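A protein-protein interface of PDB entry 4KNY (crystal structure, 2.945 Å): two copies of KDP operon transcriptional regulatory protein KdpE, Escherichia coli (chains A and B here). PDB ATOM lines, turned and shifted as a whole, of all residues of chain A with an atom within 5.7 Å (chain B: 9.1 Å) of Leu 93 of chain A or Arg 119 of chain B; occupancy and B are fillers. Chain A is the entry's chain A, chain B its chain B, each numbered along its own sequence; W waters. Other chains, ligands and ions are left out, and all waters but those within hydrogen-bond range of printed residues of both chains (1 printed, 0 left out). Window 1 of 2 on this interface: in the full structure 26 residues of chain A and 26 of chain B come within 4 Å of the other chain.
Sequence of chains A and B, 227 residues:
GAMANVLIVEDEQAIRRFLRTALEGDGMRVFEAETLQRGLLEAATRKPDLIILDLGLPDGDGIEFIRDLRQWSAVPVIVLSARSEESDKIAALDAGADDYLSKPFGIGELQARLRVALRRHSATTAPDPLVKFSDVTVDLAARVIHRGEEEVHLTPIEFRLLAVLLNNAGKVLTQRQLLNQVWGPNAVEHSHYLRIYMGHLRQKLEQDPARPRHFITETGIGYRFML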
ATOM      1  N   ASP A  88      14.405 -36.861   2.522  1.00  0.00           N
ATOM      2  CA  ASP A  88      13.302 -37.799   2.353  1.00  0.00           C
ATOM      3  C   ASP A  88      12.152 -37.471   3.301  1.00  0.00           C
ATOM      4  O   ASP A  88      10.981 -37.526   2.915  1.00  0.00           O
ATOM      5  CB  ASP A  88      13.785 -39.234   2.573  1.00  0.00           C
ATOM      6  CG  ASP A  88      12.737 -40.265   2.203  1.00  0.00           C
ATOM      7  OD1 ASP A  88      11.837 -39.935   1.402  1.00  0.00           O
ATOM      8  OD2 ASP A  88      12.818 -41.404   2.709  1.00  0.00           O
ATOM      9  N   LYS A  89      12.494 -37.135   4.542  1.00  0.00           N
ATOM     10  CA  LYS A  89      11.506 -36.703   5.523  1.00  0.00           C
ATOM     11  C   LYS A  89      10.736 -35.502   5.000  1.00  0.00           C
ATOM     12  O   LYS A  89       9.506 -35.507   4.967  1.00  0.00           O
ATOM     13  CB  LYS A  89      12.180 -36.329   6.845  1.00  0.00           C
ATOM     14  CG  LYS A  89      12.733 -37.496   7.634  1.00  0.00           C
ATOM     15  CD  LYS A  89      13.255 -37.031   8.986  1.00  0.00           C
ATOM     16  CE  LYS A  89      13.795 -38.187   9.814  1.00  0.00           C
ATOM     17  NZ  LYS A  89      14.381 -37.718  11.100  1.00  0.00           N
ATOM     18  N   ILE A  90      11.475 -34.479   4.583  1.00  0.00           N
ATOM     19  CA  ILE A  90      10.878 -33.249   4.073  1.00  0.00           C
ATOM     20  C   ILE A  90      10.001 -33.504   2.849  1.00  0.00           C
ATOM     21  O   ILE A  90       8.903 -32.956   2.736  1.00  0.00           O
ATOM     22  CB  ILE A  90      11.961 -32.209   3.730  1.00  0.00           C
ATOM     23  CG1 ILE A  90      12.764 -31.852   4.983  1.00  0.00           C
ATOM     24  CG2 ILE A  90      11.339 -30.963   3.132  1.00  0.00           C
ATOM     25  CD1 ILE A  90      13.912 -30.905   4.725  1.00  0.00           C
ATOM     26  N   ALA A  91      10.484 -34.345   1.940  1.00  0.00           N
ATOM     27  CA  ALA A  91       9.738 -34.666   0.726  1.00  0.00           C
ATOM     28  C   ALA A  91       8.420 -35.363   1.055  1.00  0.00           C
ATOM     29  O   ALA A  91       7.357 -34.969   0.567  1.00  0.00           O
ATOM     30  CB  ALA A  91      10.579 -35.529  -0.201  1.00  0.00           C
ATOM     31  N   ALA A  92       8.497 -36.395   1.890  1.00  0.00           N
ATOM     32  CA  ALA A  92       7.315 -37.154   2.283  1.00  0.00           C
ATOM     33  C   ALA A  92       6.302 -36.288   3.028  1.00  0.00           C
ATOM     34  O   ALA A  92       5.100 -36.369   2.774  1.00  0.00           O
ATOM     35  CB  ALA A  92       7.712 -38.353   3.126  1.00  0.00           C
ATOM     36  N   LEU A  93       6.792 -35.460   3.945  1.00  0.00           N
ATOM     37  CA  LEU A  93       5.922 -34.601   4.743  1.00  0.00           C
ATOM     38  C   LEU A  93       5.258 -33.512   3.905  1.00  0.00           C
ATOM     39  O   LEU A  93       4.093 -33.182   4.121  1.00  0.00           O
ATOM     40  CB  LEU A  93       6.693 -33.977   5.909  1.00  0.00           C
ATOM     41  CG  LEU A  93       7.130 -34.933   7.020  1.00  0.00           C
ATOM     42  CD1 LEU A  93       7.796 -34.167   8.150  1.00  0.00           C
ATOM     43  CD2 LEU A  93       5.949 -35.740   7.535  1.00  0.00           C
ATOM     44  N   ASP A  94       6.001 -32.955   2.953  1.00  0.00           N
ATOM     45  CA  ASP A  94       5.452 -31.928   2.075  1.00  0.00           C
ATOM     46  C   ASP A  94       4.527 -32.531   1.026  1.00  0.00           C
ATOM     47  O   ASP A  94       3.689 -31.835   0.453  1.00  0.00           O
ATOM     48  CB  ASP A  94       6.566 -31.126   1.401  1.00  0.00           C
ATOM     49  CG  ASP A  94       7.279 -30.195   2.363  1.00  0.00           C
ATOM     50  OD1 ASP A  94       6.706 -29.886   3.430  1.00  0.00           O
ATOM     51  OD2 ASP A  94       8.410 -29.766   2.050  1.00  0.00           O
ATOM     52  N   ALA A  95       4.682 -33.827   0.777  1.00  0.00           N
ATOM     53  CA  ALA A  95       3.799 -34.525  -0.148  1.00  0.00           C
ATOM     54  C   ALA A  95       2.408 -34.702   0.459  1.00  0.00           C
ATOM     55  O   ALA A  95       1.411 -34.764  -0.261  1.00  0.00           O
ATOM     56  CB  ALA A  95       4.388 -35.869  -0.539  1.00  0.00           C
ATOM     57  N   GLY A  96       2.346 -34.782   1.784  1.00  0.00           N
ATOM     58  CA  GLY A  96       1.074 -34.881   2.474  1.00  0.00           C
ATOM     59  C   GLY A  96       1.075 -35.796   3.685  1.00  0.00           C
ATOM     60  O   GLY A  96       0.041 -35.986   4.325  1.00  0.00           O
ATOM     61  N   ALA A  97       2.231 -36.369   4.001  1.00  0.00           N
ATOM     62  CA  ALA A  97       2.347 -37.238   5.166  1.00  0.00           C
ATOM     63  C   ALA A  97       2.147 -36.449   6.453  1.00  0.00           C
ATOM     64  O   ALA A  97       2.409 -35.247   6.502  1.00  0.00           O
ATOM     65  CB  ALA A  97       3.691 -37.938   5.178  1.00  0.00           C
ATOM     66  N   ASP A  98       1.683 -37.130   7.495  1.00  0.00           N
ATOM     67  CA  ASP A  98       1.413 -36.479   8.771  1.00  0.00           C
ATOM     68  C   ASP A  98       2.514 -36.750   9.791  1.00  0.00           C
ATOM     69  O   ASP A  98       2.694 -35.983  10.738  1.00  0.00           O
ATOM     70  CB  ASP A  98       0.057 -36.928   9.321  1.00  0.00           C
ATOM     71  CG  ASP A  98      -1.089 -36.615   8.375  1.00  0.00           C
ATOM     72  OD1 ASP A  98      -1.810 -35.623   8.615  1.00  0.00           O
ATOM     73  OD2 ASP A  98      -1.264 -37.358   7.386  1.00  0.00           O
ATOM     74  N   ASP A  99       3.244 -37.843   9.598  1.00  0.00           N
ATOM     75  CA  ASP A  99       4.359 -38.172  10.478  1.00  0.00           C
ATOM     76  C   ASP A  99       5.370 -39.087   9.792  1.00  0.00           C
ATOM     77  O   ASP A  99       5.059 -39.731   8.789  1.00  0.00           O
ATOM     78  CB  ASP A  99       3.860 -38.807  11.778  1.00  0.00           C
ATOM     79  CG  ASP A  99       4.784 -38.533  12.948  1.00  0.00           C
ATOM     80  OD1 ASP A  99       6.011 -38.463  12.725  1.00  0.00           O
ATOM     81  OD2 ASP A  99       4.283 -38.372  14.082  1.00  0.00           O
ATOM     82  N   TYR A 100       6.577 -39.140  10.349  1.00  0.00           N
ATOM     83  CA  TYR A 100       7.679 -39.889   9.756  1.00  0.00           C
ATOM     84  C   TYR A 100       8.511 -40.564  10.844  1.00  0.00           C
ATOM     85  O   TYR A 100       8.915 -39.927  11.814  1.00  0.00           O
ATOM     86  CB  TYR A 100       8.558 -38.943   8.935  1.00  0.00           C
ATOM     87  CG  TYR A 100       9.568 -39.607   8.021  1.00  0.00           C
ATOM     88  CD1 TYR A 100      10.708 -40.217   8.533  1.00  0.00           C
ATOM     89  CD2 TYR A 100       9.401 -39.586   6.641  1.00  0.00           C
ATOM     90  CE1 TYR A 100      11.638 -40.810   7.698  1.00  0.00           C
ATOM     91  CE2 TYR A 100      10.328 -40.173   5.799  1.00  0.00           C
ATOM     92  CZ  TYR A 100      11.444 -40.783   6.334  1.00  0.00           C
ATOM     93  OH  TYR A 100      12.372 -41.368   5.502  1.00  0.00           O
ATOM     94  N   ALA B   4       1.744 -16.598  10.196  1.00  0.00           N
ATOM     95  CA  ALA B   4       1.511 -17.600  11.226  1.00  0.00           C
ATOM     96  C   ALA B   4       2.174 -17.175  12.531  1.00  0.00           C
ATOM     97  O   ALA B   4       3.375 -16.910  12.570  1.00  0.00           O
ATOM     98  CB  ALA B   4       2.037 -18.954  10.781  1.00  0.00           C
ATOM     99  N   MET B  28       7.323 -16.557   9.005  1.00  0.00           N
ATOM    100  CA  MET B  28       6.439 -16.659  10.162  1.00  0.00           C
ATOM    101  C   MET B  28       6.708 -15.539  11.163  1.00  0.00           C
ATOM    102  O   MET B  28       7.685 -14.800  11.038  1.00  0.00           O
ATOM    103  CB  MET B  28       6.580 -18.021  10.847  1.00  0.00           C
ATOM    104  CG  MET B  28       6.342 -19.217   9.940  1.00  0.00           C
ATOM    105  SD  MET B  28       6.051 -20.734  10.869  1.00  0.00           S
ATOM    106  CE  MET B  28       6.525 -21.979   9.673  1.00  0.00           C
ATOM    107  N   ASP B  49      -0.901 -19.661  16.646  1.00  0.00           N
ATOM    108  CA  ASP B  49      -1.382 -20.726  15.782  1.00  0.00           C
ATOM    109  C   ASP B  49      -0.636 -22.022  16.075  1.00  0.00           C
ATOM    110  O   ASP B  49      -1.061 -23.098  15.662  1.00  0.00           O
ATOM    111  CB  ASP B  49      -1.214 -20.337  14.309  1.00  0.00           C
ATOM    112  CG  ASP B  49      -1.882 -19.015  13.972  1.00  0.00           C
ATOM    113  OD1 ASP B  49      -3.120 -18.996  13.822  1.00  0.00           O
ATOM    114  OD2 ASP B  49      -1.165 -17.998  13.860  1.00  0.00           O
ATOM    115  N   LEU B  50       0.470 -21.905  16.804  1.00  0.00           N
ATOM    116  CA  LEU B  50       1.333 -23.042  17.097  1.00  0.00           C
ATOM    117  C   LEU B  50       2.305 -22.720  18.229  1.00  0.00           C
ATOM    118  O   LEU B  50       2.829 -21.611  18.306  1.00  0.00           O
ATOM    119  CB  LEU B  50       2.106 -23.447  15.839  1.00  0.00           C
ATOM    120  CG  LEU B  50       3.281 -24.423  15.952  1.00  0.00           C
ATOM    121  CD1 LEU B  50       2.822 -25.775  16.454  1.00  0.00           C
ATOM    122  CD2 LEU B  50       3.961 -24.562  14.605  1.00  0.00           C
ATOM    123  N   PRO B  76      -1.976 -26.497  18.217  1.00  0.00           N
ATOM    124  CA  PRO B  76      -0.896 -27.456  17.975  1.00  0.00           C
ATOM    125  C   PRO B  76       0.338 -27.117  18.801  1.00  0.00           C
ATOM    126  O   PRO B  76       0.758 -25.959  18.828  1.00  0.00           O
ATOM    127  CB  PRO B  76      -0.590 -27.265  16.487  1.00  0.00           C
ATOM    128  CG  PRO B  76      -1.869 -26.788  15.903  1.00  0.00           C
ATOM    129  CD  PRO B  76      -2.506 -25.933  16.962  1.00  0.00           C
ATOM    130  N   ASP B  99       3.527 -33.269  18.084  1.00  0.00           N
ATOM    131  CA  ASP B  99       4.766 -33.807  17.535  1.00  0.00           C
ATOM    132  C   ASP B  99       5.916 -33.701  18.535  1.00  0.00           C
ATOM    133  O   ASP B  99       5.855 -32.931  19.494  1.00  0.00           O
ATOM    134  CB  ASP B  99       5.128 -33.107  16.222  1.00  0.00           C
ATOM    135  CG  ASP B  99       6.040 -33.947  15.342  1.00  0.00           C
ATOM    136  OD1 ASP B  99       6.672 -34.894  15.860  1.00  0.00           O
ATOM    137  OD2 ASP B  99       6.128 -33.660  14.131  1.00  0.00           O
ATOM    138  N   LEU B 101      10.298 -33.748  18.629  1.00  0.00           N
ATOM    139  CA  LEU B 101      11.599 -33.756  17.974  1.00  0.00           C
ATOM    140  C   LEU B 101      12.722 -33.919  18.992  1.00  0.00           C
ATOM    141  O   LEU B 101      12.810 -33.165  19.966  1.00  0.00           O
ATOM    142  CB  LEU B 101      11.816 -32.472  17.168  1.00  0.00           C
ATOM    143  CG  LEU B 101      11.114 -32.324  15.816  1.00  0.00           C
ATOM    144  CD1 LEU B 101       9.627 -32.060  15.985  1.00  0.00           C
ATOM    145  CD2 LEU B 101      11.766 -31.220  14.999  1.00  0.00           C
ATOM    146  N   GLY B 108      15.528 -27.870   8.416  1.00  0.00           N
ATOM    147  CA  GLY B 108      14.621 -28.254   7.351  1.00  0.00           C
ATOM    148  C   GLY B 108      13.481 -29.131   7.827  1.00  0.00           C
ATOM    149  O   GLY B 108      12.316 -28.860   7.526  1.00  0.00           O
ATOM    150  N   GLU B 109      13.812 -30.183   8.571  1.00  0.00           N
ATOM    151  CA  GLU B 109      12.795 -31.083   9.102  1.00  0.00           C
ATOM    152  C   GLU B 109      11.873 -30.339  10.053  1.00  0.00           C
ATOM    153  O   GLU B 109      10.662 -30.565  10.057  1.00  0.00           O
ATOM    154  CB  GLU B 109      13.426 -32.274   9.822  1.00  0.00           C
ATOM    155  CG  GLU B 109      12.395 -33.236  10.395  1.00  0.00           C
ATOM    156  CD  GLU B 109      12.999 -34.272  11.321  1.00  0.00           C
ATOM    157  OE1 GLU B 109      14.226 -34.494  11.255  1.00  0.00           O
ATOM    158  OE2 GLU B 109      12.240 -34.860  12.121  1.00  0.00           O
ATOM    159  N   LEU B 110      12.451 -29.449  10.853  1.00  0.00           N
ATOM    160  CA  LEU B 110      11.663 -28.637  11.770  1.00  0.00           C
ATOM    161  C   LEU B 110      10.641 -27.818  10.998  1.00  0.00           C
ATOM    162  O   LEU B 110       9.447 -27.894  11.283  1.00  0.00           O
ATOM    163  CB  LEU B 110      12.553 -27.723  12.612  1.00  0.00           C
ATOM    164  CG  LEU B 110      11.794 -26.809  13.576  1.00  0.00           C
ATOM    165  CD1 LEU B 110      10.924 -27.625  14.516  1.00  0.00           C
ATOM    166  CD2 LEU B 110      12.755 -25.935  14.363  1.00  0.00           C
ATOM    167  N   GLN B 111      11.110 -27.052  10.013  1.00  0.00           N
ATOM    168  CA  GLN B 111      10.213 -26.253   9.177  1.00  0.00           C
ATOM    169  C   GLN B 111       9.116 -27.102   8.529  1.00  0.00           C
ATOM    170  O   GLN B 111       7.945 -26.706   8.494  1.00  0.00           O
ATOM    171  CB  GLN B 111      11.008 -25.500   8.107  1.00  0.00           C
ATOM    172  CG  GLN B 111      11.866 -24.372   8.658  1.00  0.00           C
ATOM    173  CD  GLN B 111      12.805 -23.791   7.620  1.00  0.00           C
ATOM    174  OE1 GLN B 111      13.059 -24.405   6.583  1.00  0.00           O
ATOM    175  NE2 GLN B 111      13.326 -22.601   7.893  1.00  0.00           N
ATOM    176  N   ALA B 112       9.502 -28.275   8.034  1.00  0.00           N
ATOM    177  CA  ALA B 112       8.557 -29.201   7.417  1.00  0.00           C
ATOM    178  C   ALA B 112       7.451 -29.609   8.387  1.00  0.00           C
ATOM    179  O   ALA B 112       6.262 -29.533   8.061  1.00  0.00           O
ATOM    180  CB  ALA B 112       9.284 -30.429   6.895  1.00  0.00           C
ATOM    181  N   ARG B 113       7.848 -30.036   9.581  1.00  0.00           N
ATOM    182  CA  ARG B 113       6.891 -30.462  10.593  1.00  0.00           C
ATOM    183  C   ARG B 113       6.000 -29.311  11.059  1.00  0.00           C
ATOM    184  O   ARG B 113       4.825 -29.513  11.371  1.00  0.00           O
ATOM    185  CB  ARG B 113       7.613 -31.117  11.774  1.00  0.00           C
ATOM    186  CG  ARG B 113       8.347 -32.393  11.394  1.00  0.00           C
ATOM    187  CD  ARG B 113       8.900 -33.115  12.605  1.00  0.00           C
ATOM    188  NE  ARG B 113       9.373 -34.452  12.260  1.00  0.00           N
ATOM    189  CZ  ARG B 113       8.593 -35.528  12.215  1.00  0.00           C
ATOM    190  NH1 ARG B 113       7.301 -35.425  12.496  1.00  0.00           N
ATOM    191  NH2 ARG B 113       9.103 -36.707  11.889  1.00  0.00           N
ATOM    192  N   LEU B 114       6.563 -28.105  11.099  1.00  0.00           N
ATOM    193  CA  LEU B 114       5.781 -26.910  11.397  1.00  0.00           C
ATOM    194  C   LEU B 114       4.685 -26.748  10.350  1.00  0.00           C
ATOM    195  O   LEU B 114       3.519 -26.527  10.688  1.00  0.00           O
ATOM    196  CB  LEU B 114       6.668 -25.663  11.411  1.00  0.00           C
ATOM    197  CG  LEU B 114       7.809 -25.596  12.426  1.00  0.00           C
ATOM    198  CD1 LEU B 114       8.709 -24.407  12.136  1.00  0.00           C
ATOM    199  CD2 LEU B 114       7.287 -25.539  13.848  1.00  0.00           C
ATOM    200  N   ARG B 115       5.069 -26.863   9.080  1.00  0.00           N
ATOM    201  CA  ARG B 115       4.104 -26.797   7.985  1.00  0.00           C
ATOM    202  C   ARG B 115       3.016 -27.858   8.128  1.00  0.00           C
ATOM    203  O   ARG B 115       1.843 -27.585   7.874  1.00  0.00           O
ATOM    204  CB  ARG B 115       4.800 -26.942   6.630  1.00  0.00           C
ATOM    205  CG  ARG B 115       5.585 -25.717   6.200  1.00  0.00           C
ATOM    206  CD  ARG B 115       5.983 -25.802   4.738  1.00  0.00           C
ATOM    207  NE  ARG B 115       6.853 -26.943   4.468  1.00  0.00           N
ATOM    208  CZ  ARG B 115       8.177 -26.910   4.568  1.00  0.00           C
ATOM    209  NH1 ARG B 115       8.787 -25.793   4.939  1.00  0.00           N
ATOM    210  NH2 ARG B 115       8.893 -27.994   4.301  1.00  0.00           N
ATOM    211  N   VAL B 116       3.409 -29.061   8.533  1.00  0.00           N
ATOM    212  CA  VAL B 116       2.451 -30.141   8.753  1.00  0.00           C
ATOM    213  C   VAL B 116       1.440 -29.776   9.839  1.00  0.00           C
ATOM    214  O   VAL B 116       0.235 -29.930   9.653  1.00  0.00           O
ATOM    215  CB  VAL B 116       3.156 -31.459   9.134  1.00  0.00           C
ATOM    216  CG1 VAL B 116       2.139 -32.499   9.577  1.00  0.00           C
ATOM    217  CG2 VAL B 116       3.981 -31.977   7.967  1.00  0.00           C
ATOM    218  N   ALA B 117       1.940 -29.278  10.965  1.00  0.00           N
ATOM    219  CA  ALA B 117       1.079 -28.915  12.086  1.00  0.00           C
ATOM    220  C   ALA B 117       0.183 -27.717  11.779  1.00  0.00           C
ATOM    221  O   ALA B 117      -0.883 -27.564  12.375  1.00  0.00           O
ATOM    222  CB  ALA B 117       1.914 -28.644  13.328  1.00  0.00           C
ATOM    223  N   LEU B 118       0.617 -26.866  10.853  1.00  0.00           N
ATOM    224  CA  LEU B 118      -0.111 -25.634  10.556  1.00  0.00           C
ATOM    225  C   LEU B 118      -1.171 -25.775   9.465  1.00  0.00           C
ATOM    226  O   LEU B 118      -2.142 -25.020   9.441  1.00  0.00           O
ATOM    227  CB  LEU B 118       0.863 -24.510  10.189  1.00  0.00           C
ATOM    228  CG  LEU B 118       1.645 -23.884  11.346  1.00  0.00           C
ATOM    229  CD1 LEU B 118       2.563 -22.779  10.843  1.00  0.00           C
ATOM    230  CD2 LEU B 118       0.692 -23.355  12.407  1.00  0.00           C
ATOM    231  N   ARG B 119      -0.994 -26.742   8.570  1.00  0.00           N
ATOM    232  CA  ARG B 119      -1.882 -26.878   7.417  1.00  0.00           C
ATOM    233  C   ARG B 119      -3.207 -27.565   7.741  1.00  0.00           C
ATOM    234  O   ARG B 119      -3.966 -27.914   6.837  1.00  0.00           O
ATOM    235  CB  ARG B 119      -1.178 -27.610   6.272  1.00  0.00           C
ATOM    236  CG  ARG B 119      -0.900 -29.077   6.548  1.00  0.00           C
ATOM    237  CD  ARG B 119       0.043 -29.653   5.500  1.00  0.00           C
ATOM    238  NE  ARG B 119       0.329 -31.063   5.739  1.00  0.00           N
ATOM    239  CZ  ARG B 119       1.391 -31.700   5.255  1.00  0.00           C
ATOM    240  NH1 ARG B 119       2.278 -31.049   4.511  1.00  0.00           N
ATOM    241  NH2 ARG B 119       1.573 -32.987   5.520  1.00  0.00           N
ATOM    242  N   ARG B 120      -3.485 -27.755   9.026  1.00  0.00           N
ATOM    243  CA  ARG B 120      -4.751 -28.342   9.444  1.00  0.00           C
ATOM    244  C   ARG B 120      -5.799 -27.260   9.683  1.00  0.00           C
ATOM    245  O   ARG B 120      -6.983 -27.457   9.408  1.00  0.00           O
ATOM    246  CB  ARG B 120      -4.572 -29.187  10.706  1.00  0.00           C
ATOM    247  CG  ARG B 120      -3.489 -30.245  10.594  1.00  0.00           C
ATOM    248  CD  ARG B 120      -3.639 -31.307  11.671  1.00  0.00           C
ATOM    249  NE  ARG B 120      -2.536 -32.264  11.652  1.00  0.00           N
ATOM    250  CZ  ARG B 120      -2.435 -33.273  10.792  1.00  0.00           C
ATOM    251  NH1 ARG B 120      -3.370 -33.458   9.868  1.00  0.00           N
ATOM    252  NH2 ARG B 120      -1.395 -34.094  10.852  1.00  0.00           N
ATOM    253  N   HIS B 121      -5.352 -26.114  10.188  1.00  0.00           N
ATOM    254  CA  HIS B 121      -6.252 -25.011  10.504  1.00  0.00           C
ATOM    255  C   HIS B 121      -5.924 -23.772   9.677  1.00  0.00           C
ATOM    256  O   HIS B 121      -6.819 -23.120   9.138  1.00  0.00           O
ATOM    257  CB  HIS B 121      -6.173 -24.672  11.994  1.00  0.00           C
ATOM    258  CG  HIS B 121      -5.995 -25.865  12.878  1.00  0.00           C
ATOM    259  ND1 HIS B 121      -7.058 -26.589  13.378  1.00  0.00           N
ATOM    260  CD2 HIS B 121      -4.878 -26.463  13.354  1.00  0.00           C
ATOM    261  CE1 HIS B 121      -6.600 -27.580  14.122  1.00  0.00           C
ATOM    262  NE2 HIS B 121      -5.280 -27.527  14.124  1.00  0.00           N
ATOM    263  N   SER B 122      -4.636 -23.456   9.575  1.00  0.00           N
ATOM    264  CA  SER B 122      -4.192 -22.252   8.876  1.00  0.00           C
ATOM    265  C   SER B 122      -4.236 -22.400   7.356  1.00  0.00           C
ATOM    266  O   SER B 122      -3.848 -21.488   6.625  1.00  0.00           O
ATOM    267  CB  SER B 122      -2.785 -21.849   9.329  1.00  0.00           C
ATOM    268  OG  SER B 122      -2.788 -21.404  10.675  1.00  0.00           O
ATOM    269  N   ALA B 123      -4.706 -23.548   6.883  1.00  0.00           N
ATOM    270  CA  ALA B 123      -4.874 -23.768   5.454  1.00  0.00           C
ATOM    271  C   ALA B 123      -6.244 -23.279   4.997  1.00  0.00           C
ATOM    272  O   ALA B 123      -7.268 -23.881   5.325  1.00  0.00           O
ATOM    273  CB  ALA B 123      -4.692 -25.241   5.118  1.00  0.00           C
ATOM    274  N   THR B 124      -6.256 -22.180   4.245  1.00  0.00           N
ATOM    275  CA  THR B 124      -7.498 -21.603   3.740  1.00  0.00           C
ATOM    276  C   THR B 124      -7.413 -21.309   2.244  1.00  0.00           C
ATOM    277  O   THR B 124      -8.330 -20.724   1.666  1.00  0.00           O
ATOM    278  CB  THR B 124      -7.853 -20.301   4.477  1.00  0.00           C
ATOM    279  OG1 THR B 124      -6.761 -19.377   4.380  1.00  0.00           O
ATOM    280  CG2 THR B 124      -8.134 -20.583   5.948  1.00  0.00           C
ATOM    281  N   THR B 125      -6.307 -21.728   1.629  1.00  0.00           N
ATOM    282  CA  THR B 125      -6.039 -21.487   0.214  1.00  0.00           C
ATOM    283  C   THR B 125      -6.135 -20.007  -0.153  1.00  0.00           C
ATOM    284  O   THR B 125      -7.124 -19.569  -0.739  1.00  0.00           O
ATOM    285  CB  THR B 125      -6.973 -22.311  -0.695  1.00  0.00           C
ATOM    286  OG1 THR B 125      -8.320 -21.834  -0.571  1.00  0.00           O
ATOM    287  CG2 THR B 125      -6.921 -23.784  -0.313  1.00  0.00           C
HETATM  288  O   HOH W   1      -0.757 -33.499   7.105  1.00  0.00           O
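1 position is printed for both chains.
Water W1 bridges the side-chain carboxylate of Asp 98 of chain A (2.8 Å) and the guanidinium group of Arg 119 of chain B (2.9 Å).
The side-chain carboxylate (OD1) of Asp 98 of chain A lies within salt-bridge range of the guanidinium group (NH2) of Arg 120 of chain B, at 2.7 Å.
The side-chain carboxylate (OD2) of Asp 94 of chain A is in salt-bridge range of the guanidinium group (NH2) of Arg 115 of chain B (2.9 Å).
NZ of Lys 89 of chain A lies within salt-bridge range of OE1 of Glu 109 of chain B (3.2 Å).
The guanidinium group (NH1) of Arg 113 of chain B is in salt-bridge range of the side-chain carboxylate (OD1) of Asp 99 of chain A (3.3 Å).
The guanidinium group (NH2) of Arg 119 of chain B sits at hydrogen-bond distance from the backbone carbonyl oxygen (O) of Ala 97 of chain A (2.6 Å).
O of Tyr 100 of chain A lies within hydrogen-bond range of NH2 of Arg 113 of chain B (3.2 Å).
The backbone carbonyl oxygen (O) of Leu 93 of chain A lies within hydrogen-bond range of the guanidinium group (NH1) of Arg 119 of chain B, at 2.8 Å.
Of chain B, only Arg 113 (3.7 Å), Val 116 (3.9 Å) and Arg 119 (2.8 Å) come within 4 Å of Leu 93 of chain A.
Printed residues of chain A within 4 Å of Arg 119 of chain B: Leu 93, Gly 96 and Ala 97.
No residue of chain B comes within 4 Å of Ala 92 of chain A.
Of the printed residues of chain B, Tyr 100 of chain A touches Arg 113 (3.2 Å).
Printed residues of chain B within 4 Å of Asp 99 of chain A: Arg 113.
Of the printed residues of chain A, Arg 115 of chain B touches Asp 94.
Ala 117 of chain B touches none of the printed residues of chain A.
Leu 110 of chain B touches none of the printed residues of chain A.
The nearest residue of chain A that does not touch Arg 119 of chain B is Asp 94 of chain A (4.1 Å).
The nearest printed residue of chain B that does not touch Asp 99 of chain A is Asp 99 of chain B (4.6 Å).
Among the printed residues, pairs that only touch across the chains: Ile 90 of chain A with Gly 108 of chain B (3.6 Å), Ile 90 of chain A with Glu 109 of chain B (3.9 Å), Leu 93 of chain A with Arg 113 of chain B (3.7 Å), Leu 93 of chain A with Val 116 of chain B (3.9 Å), Gly 96 of chain A with Arg 119 of chain B (3.4 Å), Ala 97 of chain A with Val 116 of chain B (3.9 Å) and Asp 98 of chain A with Val 116 of chain B (3.7 Å).
NE of Arg 113 of chain B is in salt-bridge range of OE2 of Glu 109 of chain B, 2.9 Å away.
The side-chain carboxylate (OD2) of Asp 99 of chain B lies within salt-bridge range of the guanidinium group (NH1) of Arg 113 of chain B, 2.7 Å away.
The backbone carbonyl oxygen (O) of Ala 92 of chain A lies within hydrogen-bond range of the backbone NH (N) of Ala 97 of chain A (3.1 Å).
The side-chain carboxylate (OD2) of Asp 88 of chain A sits at hydrogen-bond distance from the side-chain hydroxyl (OH) of Tyr 100 of chain A (2.8 Å).
Of the 13 printed residues of chain A, 9 touch a printed residue of chain B.
Among the printed residues, Asp or Glu carboxylates within 4 Å of a Lys or Arg side-chain nitrogen of the other chain: Lys 89 of chain A with Glu 109 of chain B, Asp 94 of chain A with Arg 115 of chain B, Asp 98 of chain A with Arg 120 of chain B and Asp 99 of chain A with Arg 113 of chain B.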
